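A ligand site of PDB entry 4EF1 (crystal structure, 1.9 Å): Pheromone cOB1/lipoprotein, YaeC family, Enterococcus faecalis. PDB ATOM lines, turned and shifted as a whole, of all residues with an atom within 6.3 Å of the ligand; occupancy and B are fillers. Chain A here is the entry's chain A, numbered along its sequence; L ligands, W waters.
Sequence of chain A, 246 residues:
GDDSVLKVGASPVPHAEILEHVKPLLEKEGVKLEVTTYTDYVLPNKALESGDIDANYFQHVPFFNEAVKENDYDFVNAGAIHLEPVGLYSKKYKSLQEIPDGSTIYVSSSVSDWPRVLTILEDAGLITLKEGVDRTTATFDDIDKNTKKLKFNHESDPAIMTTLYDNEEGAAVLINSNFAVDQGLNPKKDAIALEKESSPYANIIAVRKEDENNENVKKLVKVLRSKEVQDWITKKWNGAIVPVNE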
ATOM      1  N   SER A  11     -29.486 -26.170   9.084  1.00  0.00           N
ATOM      2  CA  SER A  11     -28.353 -26.380   9.949  1.00  0.00           C
ATOM      3  C   SER A  11     -28.569 -25.397  11.117  1.00  0.00           C
ATOM      4  O   SER A  11     -29.204 -24.354  10.888  1.00  0.00           O
ATOM      5  CB  SER A  11     -27.050 -26.067   9.250  1.00  0.00           C
ATOM      6  OG  SER A  11     -26.763 -26.953   8.152  1.00  0.00           O
ATOM      7  N   PRO A  14     -25.396 -20.715  10.564  1.00  0.00           N
ATOM      8  CA  PRO A  14     -26.301 -19.593  10.809  1.00  0.00           C
ATOM      9  C   PRO A  14     -27.744 -19.875  10.363  1.00  0.00           C
ATOM     10  O   PRO A  14     -28.633 -19.158  10.733  1.00  0.00           O
ATOM     11  CB  PRO A  14     -25.729 -18.510   9.891  1.00  0.00           C
ATOM     12  CG  PRO A  14     -25.178 -19.280   8.737  1.00  0.00           C
ATOM     13  CD  PRO A  14     -24.617 -20.519   9.339  1.00  0.00           C
ATOM     14  N   HIS A  15     -27.967 -20.935   9.619  1.00  0.00           N
ATOM     15  CA  HIS A  15     -29.255 -21.119   8.935  1.00  0.00           C
ATOM     16  C   HIS A  15     -30.480 -21.019   9.811  1.00  0.00           C
ATOM     17  O   HIS A  15     -31.359 -20.199   9.550  1.00  0.00           O
ATOM     18  CB  HIS A  15     -29.282 -22.419   8.141  1.00  0.00           C
ATOM     19  CG  HIS A  15     -28.072 -22.626   7.274  1.00  0.00           C
ATOM     20  ND1 HIS A  15     -26.837 -22.828   7.786  1.00  0.00           N
ATOM     21  CD2 HIS A  15     -27.935 -22.696   5.916  1.00  0.00           C
ATOM     22  CE1 HIS A  15     -25.957 -22.977   6.814  1.00  0.00           C
ATOM     23  NE2 HIS A  15     -26.618 -22.910   5.657  1.00  0.00           N
ATOM     24  N   TYR A  41     -25.778 -33.603   6.900  1.00  0.00           N
ATOM     25  CA  TYR A  41     -26.031 -33.171   5.537  1.00  0.00           C
ATOM     26  C   TYR A  41     -26.843 -34.180   4.708  1.00  0.00           C
ATOM     27  O   TYR A  41     -27.058 -33.945   3.536  1.00  0.00           O
ATOM     28  CB  TYR A  41     -24.707 -32.839   4.797  1.00  0.00           C
ATOM     29  CG  TYR A  41     -23.877 -31.620   5.208  1.00  0.00           C
ATOM     30  CD1 TYR A  41     -24.366 -30.640   6.061  1.00  0.00           C
ATOM     31  CD2 TYR A  41     -22.572 -31.450   4.683  1.00  0.00           C
ATOM     32  CE1 TYR A  41     -23.608 -29.532   6.398  1.00  0.00           C
ATOM     33  CE2 TYR A  41     -21.826 -30.349   5.021  1.00  0.00           C
ATOM     34  CZ  TYR A  41     -22.339 -29.400   5.885  1.00  0.00           C
ATOM     35  OH  TYR A  41     -21.599 -28.289   6.216  1.00  0.00           O
ATOM     36  N   PHE A  58     -29.579 -25.515   3.845  1.00  0.00           N
ATOM     37  CA  PHE A  58     -28.326 -26.051   4.407  1.00  0.00           C
ATOM     38  C   PHE A  58     -27.225 -26.308   3.364  1.00  0.00           C
ATOM     39  O   PHE A  58     -26.066 -26.403   3.737  1.00  0.00           O
ATOM     40  CB  PHE A  58     -28.605 -27.351   5.204  1.00  0.00           C
ATOM     41  CG  PHE A  58     -28.633 -28.581   4.335  1.00  0.00           C
ATOM     42  CD1 PHE A  58     -29.737 -28.878   3.561  1.00  0.00           C
ATOM     43  CD2 PHE A  58     -27.559 -29.442   4.316  1.00  0.00           C
ATOM     44  CE1 PHE A  58     -29.758 -29.992   2.771  1.00  0.00           C
ATOM     45  CE2 PHE A  58     -27.567 -30.568   3.512  1.00  0.00           C
ATOM     46  CZ  PHE A  58     -28.666 -30.843   2.739  1.00  0.00           C
ATOM     47  N   GLN A  59     -27.579 -26.484   2.092  1.00  0.00           N
ATOM     48  CA  GLN A  59     -26.618 -26.959   1.066  1.00  0.00           C
ATOM     49  C   GLN A  59     -26.364 -25.969  -0.046  1.00  0.00           C
ATOM     50  O   GLN A  59     -27.242 -25.156  -0.373  1.00  0.00           O
ATOM     51  CB  GLN A  59     -27.135 -28.244   0.420  1.00  0.00           C
ATOM     52  CG  GLN A  59     -28.383 -28.134  -0.430  1.00  0.00           C
ATOM     53  CD  GLN A  59     -29.100 -29.453  -0.709  1.00  0.00           C
ATOM     54  OE1 GLN A  59     -28.476 -30.469  -1.014  1.00  0.00           O
ATOM     55  NE2 GLN A  59     -30.452 -29.428  -0.611  1.00  0.00           N
ATOM     56  N   HIS A  60     -25.194 -26.114  -0.687  1.00  0.00           N
ATOM     57  CA  HIS A  60     -24.833 -25.394  -1.890  1.00  0.00           C
ATOM     58  C   HIS A  60     -25.151 -26.233  -3.122  1.00  0.00           C
ATOM     59  O   HIS A  60     -25.460 -27.403  -2.981  1.00  0.00           O
ATOM     60  CB  HIS A  60     -23.364 -24.905  -1.858  1.00  0.00           C
ATOM     61  CG  HIS A  60     -22.325 -25.979  -1.532  1.00  0.00           C
ATOM     62  ND1 HIS A  60     -22.135 -27.069  -2.318  1.00  0.00           N
ATOM     63  CD2 HIS A  60     -21.322 -25.996  -0.585  1.00  0.00           C
ATOM     64  CE1 HIS A  60     -21.097 -27.810  -1.825  1.00  0.00           C
ATOM     65  NE2 HIS A  60     -20.588 -27.152  -0.772  1.00  0.00           N
ATOM     66  N   PHE A  63     -23.279 -29.625  -3.974  1.00  0.00           N
ATOM     67  CA  PHE A  63     -23.695 -30.671  -3.072  1.00  0.00           C
ATOM     68  C   PHE A  63     -25.104 -31.153  -3.491  1.00  0.00           C
ATOM     69  O   PHE A  63     -25.351 -32.347  -3.556  1.00  0.00           O
ATOM     70  CB  PHE A  63     -23.726 -30.173  -1.633  1.00  0.00           C
ATOM     71  CG  PHE A  63     -24.095 -31.241  -0.637  1.00  0.00           C
ATOM     72  CD1 PHE A  63     -25.418 -31.518  -0.385  1.00  0.00           C
ATOM     73  CD2 PHE A  63     -23.119 -31.943   0.041  1.00  0.00           C
ATOM     74  CE1 PHE A  63     -25.773 -32.514   0.527  1.00  0.00           C
ATOM     75  CE2 PHE A  63     -23.462 -32.945   0.948  1.00  0.00           C
ATOM     76  CZ  PHE A  63     -24.794 -33.220   1.196  1.00  0.00           C
ATOM     77  N   PHE A  64     -25.998 -30.193  -3.717  1.00  0.00           N
ATOM     78  CA  PHE A  64     -27.393 -30.444  -4.156  1.00  0.00           C
ATOM     79  C   PHE A  64     -27.401 -31.370  -5.390  1.00  0.00           C
ATOM     80  O   PHE A  64     -28.147 -32.389  -5.421  1.00  0.00           O
ATOM     81  CB  PHE A  64     -28.064 -29.077  -4.447  1.00  0.00           C
ATOM     82  CG  PHE A  64     -29.449 -29.160  -5.048  1.00  0.00           C
ATOM     83  CD1 PHE A  64     -30.560 -29.343  -4.232  1.00  0.00           C
ATOM     84  CD2 PHE A  64     -29.642 -29.011  -6.413  1.00  0.00           C
ATOM     85  CE1 PHE A  64     -31.823 -29.426  -4.778  1.00  0.00           C
ATOM     86  CE2 PHE A  64     -30.911 -29.084  -6.967  1.00  0.00           C
ATOM     87  CZ  PHE A  64     -32.007 -29.297  -6.153  1.00  0.00           C
ATOM     88  N   HIS A  82     -26.907 -17.243   0.686  1.00  0.00           N
ATOM     89  CA  HIS A  82     -25.622 -16.804   1.262  1.00  0.00           C
ATOM     90  C   HIS A  82     -24.469 -17.728   0.970  1.00  0.00           C
ATOM     91  O   HIS A  82     -24.660 -18.878   0.696  1.00  0.00           O
ATOM     92  CB  HIS A  82     -25.744 -16.646   2.774  1.00  0.00           C
ATOM     93  CG  HIS A  82     -25.713 -17.959   3.552  1.00  0.00           C
ATOM     94  ND1 HIS A  82     -26.823 -18.604   3.923  1.00  0.00           N
ATOM     95  CD2 HIS A  82     -24.655 -18.678   4.060  1.00  0.00           C
ATOM     96  CE1 HIS A  82     -26.514 -19.662   4.629  1.00  0.00           C
ATOM     97  NE2 HIS A  82     -25.161 -19.739   4.701  1.00  0.00           N
ATOM     98  N   LEU A  83     -23.242 -17.193   1.149  1.00  0.00           N
ATOM     99  CA  LEU A  83     -21.961 -17.910   0.985  1.00  0.00           C
ATOM    100  C   LEU A  83     -21.290 -18.071   2.350  1.00  0.00           C
ATOM    101  O   LEU A  83     -21.429 -17.207   3.275  1.00  0.00           O
ATOM    102  CB  LEU A  83     -20.994 -17.075   0.119  1.00  0.00           C
ATOM    103  CG  LEU A  83     -21.466 -16.386  -1.150  1.00  0.00           C
ATOM    104  CD1 LEU A  83     -20.343 -15.656  -1.882  1.00  0.00           C
ATOM    105  CD2 LEU A  83     -22.134 -17.418  -2.058  1.00  0.00           C
ATOM    106  N   GLU A  84     -20.533 -19.173   2.480  1.00  0.00           N
ATOM    107  CA  GLU A  84     -19.720 -19.450   3.664  1.00  0.00           C
ATOM    108  C   GLU A  84     -18.288 -19.806   3.219  1.00  0.00           C
ATOM    109  O   GLU A  84     -17.962 -21.003   3.080  1.00  0.00           O
ATOM    110  CB  GLU A  84     -20.296 -20.677   4.391  1.00  0.00           C
ATOM    111  CG  GLU A  84     -21.641 -20.444   4.997  1.00  0.00           C
ATOM    112  CD  GLU A  84     -22.159 -21.657   5.755  1.00  0.00           C
ATOM    113  OE1 GLU A  84     -21.410 -22.671   6.044  1.00  0.00           O
ATOM    114  OE2 GLU A  84     -23.356 -21.578   6.051  1.00  0.00           O
ATOM    115  N   VAL A  86     -14.991 -21.125   3.086  1.00  0.00           N
ATOM    116  CA  VAL A  86     -14.540 -22.229   3.913  1.00  0.00           C
ATOM    117  C   VAL A  86     -13.057 -22.059   4.302  1.00  0.00           C
ATOM    118  O   VAL A  86     -12.210 -21.567   3.528  1.00  0.00           O
ATOM    119  CB  VAL A  86     -14.773 -23.576   3.174  1.00  0.00           C
ATOM    120  CG1 VAL A  86     -13.812 -23.712   1.994  1.00  0.00           C
ATOM    121  CG2 VAL A  86     -14.699 -24.762   4.139  1.00  0.00           C
ATOM    122  N   SER A 110     -17.301 -35.392   1.767  1.00  0.00           N
ATOM    123  CA  SER A 110     -18.209 -34.747   0.845  1.00  0.00           C
ATOM    124  C   SER A 110     -17.406 -34.247  -0.356  1.00  0.00           C
ATOM    125  O   SER A 110     -16.731 -33.229  -0.284  1.00  0.00           O
ATOM    126  CB  SER A 110     -18.997 -33.608   1.509  1.00  0.00           C
ATOM    127  OG  SER A 110     -19.932 -32.999   0.613  1.00  0.00           O
ATOM    128  N   SER A 112     -18.054 -32.846  -3.173  1.00  0.00           N
ATOM    129  CA  SER A 112     -18.293 -31.532  -3.746  1.00  0.00           C
ATOM    130  C   SER A 112     -17.536 -30.380  -3.034  1.00  0.00           C
ATOM    131  O   SER A 112     -17.456 -29.293  -3.599  1.00  0.00           O
ATOM    132  CB  SER A 112     -19.784 -31.228  -3.898  1.00  0.00           C
ATOM    133  OG  SER A 112     -20.456 -31.093  -2.677  1.00  0.00           O
ATOM    134  N   ASP A 113     -17.005 -30.590  -1.818  1.00  0.00           N
ATOM    135  CA  ASP A 113     -16.162 -29.588  -1.130  1.00  0.00           C
ATOM    136  C   ASP A 113     -14.671 -29.787  -1.437  1.00  0.00           C
ATOM    137  O   ASP A 113     -13.856 -28.967  -1.041  1.00  0.00           O
ATOM    138  CB  ASP A 113     -16.354 -29.630   0.394  1.00  0.00           C
ATOM    139  CG  ASP A 113     -17.637 -28.977   0.874  1.00  0.00           C
ATOM    140  OD1 ASP A 113     -18.130 -28.037   0.211  1.00  0.00           O
ATOM    141  OD2 ASP A 113     -18.141 -29.371   1.952  1.00  0.00           O
ATOM    142  N   ARG A 116     -12.622 -27.004  -3.116  1.00  0.00           N
ATOM    143  CA  ARG A 116     -12.440 -25.843  -2.263  1.00  0.00           C
ATOM    144  C   ARG A 116     -11.102 -25.887  -1.497  1.00  0.00           C
ATOM    145  O   ARG A 116     -10.419 -24.884  -1.426  1.00  0.00           O
ATOM    146  CB  ARG A 116     -13.611 -25.735  -1.296  1.00  0.00           C
ATOM    147  CG  ARG A 116     -14.995 -25.716  -1.954  1.00  0.00           C
ATOM    148  CD  ARG A 116     -16.152 -25.619  -1.001  1.00  0.00           C
ATOM    149  NE  ARG A 116     -16.420 -24.263  -0.490  1.00  0.00           N
ATOM    150  CZ  ARG A 116     -17.370 -23.988   0.393  1.00  0.00           C
ATOM    151  NH1 ARG A 116     -18.200 -24.948   0.824  1.00  0.00           N
ATOM    152  NH2 ARG A 116     -17.545 -22.739   0.800  1.00  0.00           N
ATOM    153  N   ASN A 176     -16.522 -26.934   7.366  1.00  0.00           N
ATOM    154  CA  ASN A 176     -17.563 -26.089   6.767  1.00  0.00           C
ATOM    155  C   ASN A 176     -17.928 -25.026   7.829  1.00  0.00           C
ATOM    156  O   ASN A 176     -18.037 -25.313   9.018  1.00  0.00           O
ATOM    157  CB  ASN A 176     -18.831 -26.869   6.352  1.00  0.00           C
ATOM    158  CG  ASN A 176     -18.555 -27.942   5.320  1.00  0.00           C
ATOM    159  OD1 ASN A 176     -18.255 -29.084   5.684  1.00  0.00           O
ATOM    160  ND2 ASN A 176     -18.743 -27.613   4.043  1.00  0.00           N
ATOM    161  N   SER A 177     -18.118 -23.795   7.397  1.00  0.00           N
ATOM    162  CA  SER A 177     -18.327 -22.659   8.317  1.00  0.00           C
ATOM    163  C   SER A 177     -19.512 -22.784   9.246  1.00  0.00           C
ATOM    164  O   SER A 177     -19.437 -22.299  10.367  1.00  0.00           O
ATOM    165  CB  SER A 177     -18.373 -21.344   7.581  1.00  0.00           C
ATOM    166  OG  SER A 177     -17.162 -21.127   6.899  1.00  0.00           O
ATOM    167  N   ASN A 178     -20.578 -23.450   8.794  1.00  0.00           N
ATOM    168  CA  ASN A 178     -21.753 -23.662   9.645  1.00  0.00           C
ATOM    169  C   ASN A 178     -21.353 -24.395  10.933  1.00  0.00           C
ATOM    170  O   ASN A 178     -21.713 -23.979  12.041  1.00  0.00           O
ATOM    171  CB  ASN A 178     -22.919 -24.358   8.891  1.00  0.00           C
ATOM    172  CG  ASN A 178     -22.682 -25.805   8.612  1.00  0.00           C
ATOM    173  OD1 ASN A 178     -21.977 -26.152   7.671  1.00  0.00           O
ATOM    174  ND2 ASN A 178     -23.285 -26.683   9.442  1.00  0.00           N
ATOM    175  N   TYR A 201     -20.472 -21.771  -4.293  1.00  0.00           N
ATOM    176  CA  TYR A 201     -20.892 -22.469  -3.094  1.00  0.00           C
ATOM    177  C   TYR A 201     -21.937 -21.711  -2.259  1.00  0.00           C
ATOM    178  O   TYR A 201     -22.018 -21.913  -1.063  1.00  0.00           O
ATOM    179  CB  TYR A 201     -19.652 -22.839  -2.230  1.00  0.00           C
ATOM    180  CG  TYR A 201     -18.733 -23.690  -3.045  1.00  0.00           C
ATOM    181  CD1 TYR A 201     -19.064 -25.015  -3.339  1.00  0.00           C
ATOM    182  CD2 TYR A 201     -17.594 -23.121  -3.683  1.00  0.00           C
ATOM    183  CE1 TYR A 201     -18.272 -25.766  -4.196  1.00  0.00           C
ATOM    184  CE2 TYR A 201     -16.783 -23.886  -4.480  1.00  0.00           C
ATOM    185  CZ  TYR A 201     -17.117 -25.203  -4.732  1.00  0.00           C
ATOM    186  OH  TYR A 201     -16.341 -25.920  -5.554  1.00  0.00           O
ATOM    187  N   ALA A 202     -22.776 -20.933  -2.909  1.00  0.00           N
ATOM    188  CA  ALA A 202     -23.899 -20.250  -2.228  1.00  0.00           C
ATOM    189  C   ALA A 202     -24.864 -21.328  -1.684  1.00  0.00           C
ATOM    190  O   ALA A 202     -25.127 -22.336  -2.349  1.00  0.00           O
ATOM    191  CB  ALA A 202     -24.645 -19.277  -3.186  1.00  0.00           C
ATOM    192  N   ASN A 203     -25.302 -21.136  -0.471  1.00  0.00           N
ATOM    193  CA  ASN A 203     -26.262 -22.017   0.176  1.00  0.00           C
ATOM    194  C   ASN A 203     -27.667 -21.625  -0.297  1.00  0.00           C
ATOM    195  O   ASN A 203     -28.001 -20.440  -0.317  1.00  0.00           O
ATOM    196  CB  ASN A 203     -26.163 -21.945   1.688  1.00  0.00           C
ATOM    197  CG  ASN A 203     -24.969 -22.721   2.239  1.00  0.00           C
ATOM    198  OD1 ASN A 203     -25.015 -23.269   3.344  1.00  0.00           O
ATOM    199  ND2 ASN A 203     -23.884 -22.775   1.443  1.00  0.00           N
HETATM  200  N1  LIG L   1     -23.046 -24.611   4.950  1.00  0.00           N
HETATM  201  C1  LIG L   1     -22.104 -25.490   4.145  1.00  0.00           C
HETATM  202  C2  LIG L   1     -21.103 -24.686   3.317  1.00  0.00           C
HETATM  203  O1  LIG L   1     -21.486 -23.697   2.677  1.00  0.00           O
HETATM  204  O2  LIG L   1     -19.900 -25.069   3.204  1.00  0.00           O
HETATM  205  C3  LIG L   1     -22.862 -26.486   3.264  1.00  0.00           C
HETATM  206  C4  LIG L   1     -21.988 -27.518   2.550  1.00  0.00           C
HETATM  207 SE1  LIG L   1     -23.022 -28.518   1.272  1.00  0.00          SE
HETATM  208  C5  LIG L   1     -24.192 -29.551   2.502  1.00  0.00           C
HETATM  209  O   HOH W   1     -20.535 -21.779   1.154  1.00  0.00           O
HETATM  210  O   HOH W   2     -18.024 -23.498   4.460  1.00  0.00           O
HETATM  211  O   HOH W   3     -20.518 -30.783   1.912  1.00  0.00           O
HETATM  212  O   HOH W   4     -24.910 -26.125   6.296  1.00  0.00           O
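O of Glu 84 sits at hydrogen-bond distance from NH2 of Arg 116, at 2.9 Å.
OE2 of Glu 84 lies within hydrogen-bond range of NE2 of His 82, at 2.9 Å.
The side-chain amide oxygen (OD1) of Asn 203 sits close to the backbone carbonyl oxygen (O) of Phe 58 (3.3 Å).
The backbone carbonyl oxygen (O) of Tyr 201 lies within hydrogen-bond range of the side-chain amide nitrogen (ND2) of Asn 203 (3.2 Å).
OH of Tyr 41 lies close to OD1 of Asn 176 (3.5 Å).
ND2 of Asn 176 sits at hydrogen-bond distance from OD2 of Asp 113.
The side-chain amide oxygen (OD1) of Asn 178 lies within hydrogen-bond range of the side-chain hydroxyl (OH) of Tyr 41 (2.6 Å).
NE2 of His 60 lies within hydrogen-bond range of OD1 of Asp 113 (2.8 Å).
Water W1 lies within hydrogen-bond range of O1 of the ligand (2.6 Å), O of Tyr 201 (2.7 Å), N of Glu 84 (2.9 Å) and NH2 of Arg 116 (3.2 Å).
Water W2 lies within hydrogen-bond range of an oxygen (O2) of the ligand (2.8 Å), the backbone carbonyl oxygen of Glu 84 (2.9 Å) and the backbone NH of Ser 177 (3.0 Å).
Water W4 lies within hydrogen-bond range of OG of Ser 11, N1 of the ligand, O of Phe 58 and OD1 of Asn 178.
Water W3 lies within hydrogen-bond range of OG of Ser 110 and OD2 of Asp 113.
Merely in contact with the ligand: Phe 58, Tyr 41, Phe 63, His 60, His 15 and Gln 59.
Hydrophobic or aromatic side chains that line the ligand: His 15, Tyr 41, Phe 58, His 60 and Phe 63.
Of the 23 residues printed, 11 come within 4 Å of the ligand.
The nearest printed residue that does not touch the ligand is Tyr 201 (4.2 Å).
The side-chain carboxylate (OE1) of Glu 84 is in salt-bridge range of a nitrogen (N1) of the ligand (2.8 Å).
The side-chain amide nitrogen of Asn 203 sits at hydrogen-bond distance from an oxygen (O1) of the ligand, at 2.9 Å.
An oxygen (O2) of the ligand lies within hydrogen-bond range of the side-chain amide nitrogen (ND2) of Asn 176 (2.9 Å).
O2 of the ligand lies within salt-bridge range of NH1 of Arg 116, 2.9 Å away.
The side-chain amide oxygen (OD1) of Asn 178 lies within hydrogen-bond range of a nitrogen (N1) of the ligand, at 3.3 Å.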
